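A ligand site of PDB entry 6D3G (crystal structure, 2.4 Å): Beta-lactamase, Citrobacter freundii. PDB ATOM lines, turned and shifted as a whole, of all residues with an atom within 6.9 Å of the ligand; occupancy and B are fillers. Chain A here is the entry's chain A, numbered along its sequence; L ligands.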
ATOM      1  N   MET A  45      -1.790  -1.203  -7.173  1.00  0.00           N
ATOM      2  CA  MET A  45      -3.191  -0.802  -7.310  1.00  0.00           C
ATOM      3  C   MET A  45      -4.088  -1.914  -7.829  1.00  0.00           C
ATOM      4  O   MET A  45      -5.277  -1.961  -7.438  1.00  0.00           O
ATOM      5  CB  MET A  45      -3.297   0.398  -8.218  1.00  0.00           C
ATOM      6  CG  MET A  45      -2.804   1.709  -7.603  1.00  0.00           C
ATOM      7  SD  MET A  45      -3.249   3.114  -8.700  1.00  0.00           S
ATOM      8  CE  MET A  45      -1.873   3.000  -9.886  1.00  0.00           C
ATOM      9  N   GLN A  46      -3.567  -2.783  -8.699  1.00  0.00           N
ATOM     10  CA  GLN A  46      -4.391  -3.744  -9.429  1.00  0.00           C
ATOM     11  C   GLN A  46      -5.606  -3.018  -9.991  1.00  0.00           C
ATOM     12  O   GLN A  46      -5.472  -1.897 -10.519  1.00  0.00           O
ATOM     13  CB  GLN A  46      -4.827  -4.901  -8.524  1.00  0.00           C
ATOM     14  CG  GLN A  46      -3.691  -5.867  -8.170  1.00  0.00           C
ATOM     15  CD  GLN A  46      -3.168  -6.657  -9.342  1.00  0.00           C
ATOM     16  OE1 GLN A  46      -3.733  -6.633 -10.431  1.00  0.00           O
ATOM     17  NE2 GLN A  46      -2.042  -7.328  -9.143  1.00  0.00           N
ATOM     18  N   SER A  47      -6.779  -3.627  -9.857  1.00  0.00           N
ATOM     19  CA  SER A  47      -7.984  -3.113 -10.502  1.00  0.00           C
ATOM     20  C   SER A  47      -8.377  -1.716 -10.038  1.00  0.00           C
ATOM     21  O   SER A  47      -9.249  -1.106 -10.665  1.00  0.00           O
ATOM     22  CB  SER A  47      -9.162  -4.074 -10.261  1.00  0.00           C
ATOM     23  OG  SER A  47      -9.154  -5.201 -11.139  1.00  0.00           O
ATOM     24  N   VAL A  48      -7.789  -1.183  -8.957  1.00  0.00           N
ATOM     25  CA  VAL A  48      -8.229   0.138  -8.501  1.00  0.00           C
ATOM     26  C   VAL A  48      -7.943   1.204  -9.563  1.00  0.00           C
ATOM     27  O   VAL A  48      -8.722   2.154  -9.732  1.00  0.00           O
ATOM     28  CB  VAL A  48      -7.595   0.506  -7.143  1.00  0.00           C
ATOM     29  CG1 VAL A  48      -7.909   1.946  -6.793  1.00  0.00           C
ATOM     30  CG2 VAL A  48      -8.092  -0.437  -6.049  1.00  0.00           C
ATOM     31  N   LYS A  50      -8.530   1.204 -12.558  1.00  0.00           N
ATOM     32  CA  LYS A  50      -9.616   1.392 -13.512  1.00  0.00           C
ATOM     33  C   LYS A  50     -10.465   2.626 -13.194  1.00  0.00           C
ATOM     34  O   LYS A  50     -11.110   3.164 -14.117  1.00  0.00           O
ATOM     35  CB  LYS A  50     -10.481   0.124 -13.555  1.00  0.00           C
ATOM     36  CG  LYS A  50      -9.745  -1.027 -14.244  1.00  0.00           C
ATOM     37  CD  LYS A  50     -10.352  -2.362 -13.931  1.00  0.00           C
ATOM     38  CE  LYS A  50      -9.544  -3.468 -14.549  1.00  0.00           C
ATOM     39  NZ  LYS A  50      -9.808  -4.723 -13.811  1.00  0.00           N
ATOM     40  N   THR A  83      -8.752 -14.475 -18.816  1.00  0.00           N
ATOM     41  CA  THR A  83      -8.729 -13.392 -17.854  1.00  0.00           C
ATOM     42  C   THR A  83     -10.155 -13.114 -17.413  1.00  0.00           C
ATOM     43  O   THR A  83     -11.126 -13.665 -17.946  1.00  0.00           O
ATOM     44  CB  THR A  83      -8.080 -12.171 -18.471  1.00  0.00           C
ATOM     45  OG1 THR A  83      -7.736 -11.234 -17.447  1.00  0.00           O
ATOM     46  CG2 THR A  83      -9.042 -11.541 -19.495  1.00  0.00           C
ATOM     47  N   TRP A  84     -10.283 -12.263 -16.392  1.00  0.00           N
ATOM     48  CA  TRP A  84     -11.614 -11.946 -15.907  1.00  0.00           C
ATOM     49  C   TRP A  84     -12.263 -10.920 -16.815  1.00  0.00           C
ATOM     50  O   TRP A  84     -11.719  -9.831 -17.035  1.00  0.00           O
ATOM     51  CB  TRP A  84     -11.558 -11.484 -14.456  1.00  0.00           C
ATOM     52  CG  TRP A  84     -12.836 -10.849 -14.019  1.00  0.00           C
ATOM     53  CD1 TRP A  84     -13.100  -9.511 -14.054  1.00  0.00           C
ATOM     54  CD2 TRP A  84     -14.034 -11.483 -13.526  1.00  0.00           C
ATOM     55  NE1 TRP A  84     -14.369  -9.271 -13.576  1.00  0.00           N
ATOM     56  CE2 TRP A  84     -14.967 -10.456 -13.252  1.00  0.00           C
ATOM     57  CE3 TRP A  84     -14.413 -12.823 -13.264  1.00  0.00           C
ATOM     58  CZ2 TRP A  84     -16.254 -10.709 -12.753  1.00  0.00           C
ATOM     59  CZ3 TRP A  84     -15.704 -13.068 -12.763  1.00  0.00           C
ATOM     60  CH2 TRP A  84     -16.597 -12.022 -12.514  1.00  0.00           C
ATOM     61  N   SER A  85     -13.382 -11.300 -17.391  1.00  0.00           N
ATOM     62  CA  SER A  85     -14.121 -10.456 -18.314  1.00  0.00           C
ATOM     63  C   SER A  85     -15.579 -10.897 -18.378  1.00  0.00           C
ATOM     64  O   SER A  85     -15.904 -11.838 -19.109  1.00  0.00           O
ATOM     65  CB  SER A  85     -13.515 -10.510 -19.711  1.00  0.00           C
ATOM     66  OG  SER A  85     -14.131  -9.541 -20.563  1.00  0.00           O
ATOM     67  N   HIS A 110     -17.693  -3.838 -13.280  1.00  0.00           N
ATOM     68  CA  HIS A 110     -17.440  -5.262 -13.256  1.00  0.00           C
ATOM     69  C   HIS A 110     -15.962  -5.599 -13.238  1.00  0.00           C
ATOM     70  O   HIS A 110     -15.612  -6.768 -13.259  1.00  0.00           O
ATOM     71  CB  HIS A 110     -18.124  -5.912 -14.453  1.00  0.00           C
ATOM     72  CG  HIS A 110     -19.591  -5.616 -14.505  1.00  0.00           C
ATOM     73  ND1 HIS A 110     -20.527  -6.345 -13.796  1.00  0.00           N
ATOM     74  CD2 HIS A 110     -20.288  -4.666 -15.167  1.00  0.00           C
ATOM     75  CE1 HIS A 110     -21.735  -5.851 -14.028  1.00  0.00           C
ATOM     76  NE2 HIS A 110     -21.620  -4.833 -14.852  1.00  0.00           N
ATOM     77  N   SER A 111     -15.084  -4.589 -13.181  1.00  0.00           N
ATOM     78  CA  SER A 111     -13.643  -4.794 -13.050  1.00  0.00           C
ATOM     79  C   SER A 111     -13.096  -5.637 -14.200  1.00  0.00           C
ATOM     80  O   SER A 111     -12.160  -6.414 -14.021  1.00  0.00           O
ATOM     81  CB  SER A 111     -13.292  -5.429 -11.713  1.00  0.00           C
ATOM     82  OG  SER A 111     -11.942  -5.141 -11.349  1.00  0.00           O
ATOM     83  N   ASP A 112     -13.598  -5.371 -15.406  1.00  0.00           N
ATOM     84  CA  ASP A 112     -13.374  -6.260 -16.542  1.00  0.00           C
ATOM     85  C   ASP A 112     -12.010  -5.955 -17.153  1.00  0.00           C
ATOM     86  O   ASP A 112     -11.704  -4.803 -17.438  1.00  0.00           O
ATOM     87  CB  ASP A 112     -14.489  -6.037 -17.581  1.00  0.00           C
ATOM     88  CG  ASP A 112     -14.422  -7.000 -18.781  1.00  0.00           C
ATOM     89  OD1 ASP A 112     -13.497  -6.937 -19.627  1.00  0.00           O
ATOM     90  OD2 ASP A 112     -15.364  -7.792 -18.926  1.00  0.00           O
ATOM     91  N   ASN A 113     -11.209  -7.007 -17.356  1.00  0.00           N
ATOM     92  CA  ASN A 113      -9.821  -6.796 -17.782  1.00  0.00           C
ATOM     93  C   ASN A 113      -9.719  -6.532 -19.283  1.00  0.00           C
ATOM     94  O   ASN A 113      -8.863  -5.756 -19.724  1.00  0.00           O
ATOM     95  CB  ASN A 113      -8.960  -7.989 -17.363  1.00  0.00           C
ATOM     96  CG  ASN A 113      -8.536  -7.925 -15.901  1.00  0.00           C
ATOM     97  OD1 ASN A 113      -8.422  -6.837 -15.318  1.00  0.00           O
ATOM     98  ND2 ASN A 113      -8.300  -9.097 -15.285  1.00  0.00           N
ATOM     99  N   GLU A 147      -3.327  -4.405 -18.127  1.00  0.00           N
ATOM    100  CA  GLU A 147      -3.761  -5.679 -17.560  1.00  0.00           C
ATOM    101  C   GLU A 147      -2.990  -6.841 -18.165  1.00  0.00           C
ATOM    102  O   GLU A 147      -2.621  -7.772 -17.456  1.00  0.00           O
ATOM    103  CB  GLU A 147      -5.267  -5.862 -17.803  1.00  0.00           C
ATOM    104  CG  GLU A 147      -6.125  -4.948 -16.958  1.00  0.00           C
ATOM    105  CD  GLU A 147      -5.989  -5.193 -15.464  1.00  0.00           C
ATOM    106  OE1 GLU A 147      -5.317  -6.186 -15.079  1.00  0.00           O
ATOM    107  OE2 GLU A 147      -6.567  -4.404 -14.685  1.00  0.00           O
ATOM    108  N   MET A 150       0.387  -7.130 -16.709  1.00  0.00           N
ATOM    109  CA  MET A 150       0.347  -7.580 -15.331  1.00  0.00           C
ATOM    110  C   MET A 150       0.039  -9.065 -15.263  1.00  0.00           C
ATOM    111  O   MET A 150       0.561  -9.766 -14.391  1.00  0.00           O
ATOM    112  CB  MET A 150      -0.673  -6.758 -14.526  1.00  0.00           C
ATOM    113  CG  MET A 150      -0.189  -5.336 -14.228  1.00  0.00           C
ATOM    114  SD  MET A 150      -1.119  -4.519 -12.921  1.00  0.00           S
ATOM    115  CE  MET A 150      -2.678  -4.351 -13.799  1.00  0.00           C
ATOM    116  N   HIS A 151      -0.765  -9.560 -16.200  1.00  0.00           N
ATOM    117  CA  HIS A 151      -1.057 -10.980 -16.236  1.00  0.00           C
ATOM    118  C   HIS A 151       0.154 -11.775 -16.673  1.00  0.00           C
ATOM    119  O   HIS A 151       0.331 -12.925 -16.256  1.00  0.00           O
ATOM    120  CB  HIS A 151      -2.224 -11.239 -17.173  1.00  0.00           C
ATOM    121  CG  HIS A 151      -3.548 -10.845 -16.603  1.00  0.00           C
ATOM    122  ND1 HIS A 151      -3.821  -9.547 -16.201  1.00  0.00           N
ATOM    123  CD2 HIS A 151      -4.672 -11.558 -16.346  1.00  0.00           C
ATOM    124  CE1 HIS A 151      -5.060  -9.488 -15.733  1.00  0.00           C
ATOM    125  NE2 HIS A 151      -5.590 -10.692 -15.803  1.00  0.00           N
ATOM    126  N   THR A 195     -21.523  -1.321  -8.681  1.00  0.00           N
ATOM    127  CA  THR A 195     -20.738  -2.535  -8.647  1.00  0.00           C
ATOM    128  C   THR A 195     -21.225  -3.477  -7.549  1.00  0.00           C
ATOM    129  O   THR A 195     -21.717  -3.055  -6.496  1.00  0.00           O
ATOM    130  CB  THR A 195     -19.280  -2.174  -8.401  1.00  0.00           C
ATOM    131  OG1 THR A 195     -18.475  -3.358  -8.461  1.00  0.00           O
ATOM    132  CG2 THR A 195     -19.146  -1.527  -6.993  1.00  0.00           C
ATOM    133  N   THR A 197     -18.824  -5.834  -6.707  1.00  0.00           N
ATOM    134  CA  THR A 197     -17.514  -6.319  -6.262  1.00  0.00           C
ATOM    135  C   THR A 197     -17.307  -6.012  -4.784  1.00  0.00           C
ATOM    136  O   THR A 197     -17.927  -5.108  -4.211  1.00  0.00           O
ATOM    137  CB  THR A 197     -16.370  -5.671  -7.044  1.00  0.00           C
ATOM    138  OG1 THR A 197     -16.401  -4.259  -6.847  1.00  0.00           O
ATOM    139  CG2 THR A 197     -16.507  -5.914  -8.566  1.00  0.00           C
ATOM    140  N   GLY A 198     -16.454  -6.811  -4.152  1.00  0.00           N
ATOM    141  CA  GLY A 198     -15.998  -6.568  -2.806  1.00  0.00           C
ATOM    142  C   GLY A 198     -17.046  -6.173  -1.794  1.00  0.00           C
ATOM    143  O   GLY A 198     -16.886  -5.178  -1.085  1.00  0.00           O
ATOM    144  N   ARG A 201     -15.698  -5.662   1.732  1.00  0.00           N
ATOM    145  CA  ARG A 201     -14.574  -4.765   1.971  1.00  0.00           C
ATOM    146  C   ARG A 201     -15.131  -3.474   2.578  1.00  0.00           C
ATOM    147  O   ARG A 201     -15.613  -3.531   3.711  1.00  0.00           O
ATOM    148  CB  ARG A 201     -13.771  -4.576   0.699  1.00  0.00           C
ATOM    149  CG  ARG A 201     -13.166  -5.950   0.266  1.00  0.00           C
ATOM    150  CD  ARG A 201     -12.326  -5.870  -1.043  1.00  0.00           C
ATOM    151  NE  ARG A 201     -11.974  -7.201  -1.520  1.00  0.00           N
ATOM    152  CZ  ARG A 201     -11.085  -7.479  -2.463  1.00  0.00           C
ATOM    153  NH1 ARG A 201     -10.390  -6.520  -3.090  1.00  0.00           N
ATOM    154  NH2 ARG A 201     -10.886  -8.739  -2.808  1.00  0.00           N
ATOM    155  N   LYS A 215     -14.047   1.284  -5.863  1.00  0.00           N
ATOM    156  CA  LYS A 215     -13.366   0.395  -6.799  1.00  0.00           C
ATOM    157  C   LYS A 215     -12.434  -0.536  -6.022  1.00  0.00           C
ATOM    158  O   LYS A 215     -11.515  -0.080  -5.306  1.00  0.00           O
ATOM    159  CB  LYS A 215     -12.543   1.186  -7.842  1.00  0.00           C
ATOM    160  CG  LYS A 215     -11.928   0.297  -8.943  1.00  0.00           C
ATOM    161  CD  LYS A 215     -13.052  -0.318  -9.781  1.00  0.00           C
ATOM    162  CE  LYS A 215     -12.599  -1.554 -10.512  1.00  0.00           C
ATOM    163  NZ  LYS A 215     -12.616  -2.671  -9.526  1.00  0.00           N
ATOM    164  N   THR A 216     -12.621  -1.829  -6.225  1.00  0.00           N
ATOM    165  CA  THR A 216     -11.850  -2.899  -5.636  1.00  0.00           C
ATOM    166  C   THR A 216     -10.680  -3.227  -6.519  1.00  0.00           C
ATOM    167  O   THR A 216     -10.625  -2.868  -7.692  1.00  0.00           O
ATOM    168  CB  THR A 216     -12.711  -4.146  -5.505  1.00  0.00           C
ATOM    169  OG1 THR A 216     -13.207  -4.499  -6.803  1.00  0.00           O
ATOM    170  CG2 THR A 216     -13.841  -3.890  -4.546  1.00  0.00           C
ATOM    171  N   GLY A 217      -9.747  -3.974  -5.954  1.00  0.00           N
ATOM    172  CA  GLY A 217      -8.638  -4.539  -6.696  1.00  0.00           C
ATOM    173  C   GLY A 217      -8.062  -5.671  -5.882  1.00  0.00           C
ATOM    174  O   GLY A 217      -8.009  -5.566  -4.634  1.00  0.00           O
ATOM    175  N   THR A 218      -7.643  -6.739  -6.554  1.00  0.00           N
ATOM    176  CA  THR A 218      -7.100  -7.935  -5.905  1.00  0.00           C
ATOM    177  C   THR A 218      -6.073  -8.614  -6.801  1.00  0.00           C
ATOM    178  O   THR A 218      -6.329  -8.872  -7.979  1.00  0.00           O
ATOM    179  CB  THR A 218      -8.221  -8.921  -5.544  1.00  0.00           C
ATOM    180  OG1 THR A 218      -9.343  -8.230  -4.972  1.00  0.00           O
ATOM    181  CG2 THR A 218      -7.702  -9.968  -4.540  1.00  0.00           C
ATOM    182  N   SER A 219      -4.914  -8.961  -6.235  1.00  0.00           N
ATOM    183  CA  SER A 219      -4.001  -9.798  -6.979  1.00  0.00           C
ATOM    184  C   SER A 219      -4.348 -11.280  -6.757  1.00  0.00           C
ATOM    185  O   SER A 219      -5.253 -11.630  -5.983  1.00  0.00           O
ATOM    186  CB  SER A 219      -2.555  -9.463  -6.603  1.00  0.00           C
ATOM    187  OG  SER A 219      -2.230  -9.932  -5.314  1.00  0.00           O
ATOM    188  N   GLY A 220      -3.652 -12.154  -7.484  1.00  0.00           N
ATOM    189  CA  GLY A 220      -3.697 -13.568  -7.175  1.00  0.00           C
ATOM    190  C   GLY A 220      -2.786 -13.896  -6.005  1.00  0.00           C
ATOM    191  O   GLY A 220      -2.060 -13.054  -5.469  1.00  0.00           O
ATOM    192  N   ASN A 230      -7.438  -4.592  -2.187  1.00  0.00           N
ATOM    193  CA  ASN A 230      -7.652  -3.154  -2.094  1.00  0.00           C
ATOM    194  C   ASN A 230      -9.140  -2.795  -2.208  1.00  0.00           C
ATOM    195  O   ASN A 230      -9.944  -3.529  -2.797  1.00  0.00           O
ATOM    196  CB  ASN A 230      -6.875  -2.418  -3.183  1.00  0.00           C
ATOM    197  CG  ASN A 230      -5.391  -2.823  -3.230  1.00  0.00           C
ATOM    198  OD1 ASN A 230      -4.780  -3.183  -2.200  1.00  0.00           O
ATOM    199  ND2 ASN A 230      -4.818  -2.776  -4.426  1.00  0.00           N
HETATM  200  O1  LIG L   1      -7.865  -6.127  -9.540  1.00  0.00           O
HETATM  201  C1  LIG L   1      -8.707  -6.343 -10.436  1.00  0.00           C
HETATM  202  N1  LIG L   1      -8.840  -7.626 -11.037  1.00  0.00           N
HETATM  203  C2  LIG L   1      -9.808  -7.925 -12.046  1.00  0.00           C
HETATM  204  C3  LIG L   1      -7.999  -8.704 -10.628  1.00  0.00           C
HETATM  205  C4  LIG L   1      -7.025  -9.066 -11.774  1.00  0.00           C
HETATM  206  O2  LIG L   1      -6.876  -8.324 -12.739  1.00  0.00           O
HETATM  207  N2  LIG L   1      -6.242 -10.229 -11.734  1.00  0.00           N
HETATM  208  C5  LIG L   1      -8.852  -9.882 -10.128  1.00  0.00           C
HETATM  209  C6  LIG L   1     -10.168 -10.119 -10.860  1.00  0.00           C
HETATM  210  C7  LIG L   1     -10.843  -8.890 -11.496  1.00  0.00           C
HETATM  211  N3  LIG L   1     -11.716  -8.248 -10.530  1.00  0.00           N
HETATM  212  O3  LIG L   1     -11.311  -8.461  -9.182  1.00  0.00           O
HETATM  213  S1  LIG L   1     -11.558  -7.267  -8.257  1.00  0.00           S
HETATM  214  O4  LIG L   1     -10.644  -7.303  -7.050  1.00  0.00           O
HETATM  215  O5  LIG L   1     -13.010  -7.141  -7.755  1.00  0.00           O
HETATM  216  O6  LIG L   1     -11.162  -5.973  -8.905  1.00  0.00           O
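Residues that only touch the ligand: Gln 46, Lys 50, Trp 84, Glu 147, His 151, Thr 197 and Gly 217.
Hydrophobic or aromatic side chains that line the ligand: Trp 84 and His 151.
13 residues have an atom within 4 Å of the ligand: Gln 46, Ser 47, Lys 50, Trp 84, Ser 111, Asn 113, Glu 147, His 151, Thr 197, Lys 215, Thr 216, Gly 217 and Thr 218.
O1 of the ligand lies close to N of Ser 47 (2.7 Å).
The side-chain hydroxyl (OG) of Ser 47 is covalently linked to a carbon (C1) of the ligand (1.4 Å).
N of Thr 218 lies within hydrogen-bond range of O1 of the ligand, 3.1 Å away.
The side-chain hydroxyl of Thr 218 lies within hydrogen-bond range of an oxygen (O4) of the ligand, 2.6 Å away.
The side-chain hydroxyl (OG) of Ser 111 is in hydrogen-bond range of an oxygen (O6) of the ligand, at 2.7 Å.
O5 of the ligand is in hydrogen-bond range of OG1 of Thr 216, at 2.8 Å.
An oxygen (O2) of the ligand is in hydrogen-bond range of the side-chain amide nitrogen of Asn 113 (3.0 Å).
NZ of Lys 215 lies within salt-bridge range of O6 of the ligand, 3.7 Å away.
The side-chain hydroxyl (OG) of Ser 47 sits at hydrogen-bond distance from the side-chain amino group (NZ) of Lys 50 (2.8 Å).
The guanidinium group of Arg 201 lies within hydrogen-bond range of the side-chain hydroxyl of Thr 218 (2.7 Å).
O of Ser 111 sits at hydrogen-bond distance from NZ of Lys 50, at 2.9 Å.
The side-chain amino group (NZ) of Lys 215 sits at hydrogen-bond distance from the side-chain hydroxyl (OG1) of Thr 216, 3.3 Å away.
The side-chain carboxylate (OE2) of Glu 147 lies close to the side-chain amide oxygen (OD1) of Asn 113 (3.1 Å).
The side-chain amide oxygen (OD1) of Asn 113 lies within hydrogen-bond range of the side-chain amino group (NZ) of Lys 50 (2.9 Å).
The side-chain amide nitrogen (ND2) of Asn 113 is in hydrogen-bond range of a ring nitrogen (NE2) of His 151, 3.2 Å away.
NZ of Lys 50 is in salt-bridge range of OE2 of Glu 147, at 3.4 Å.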
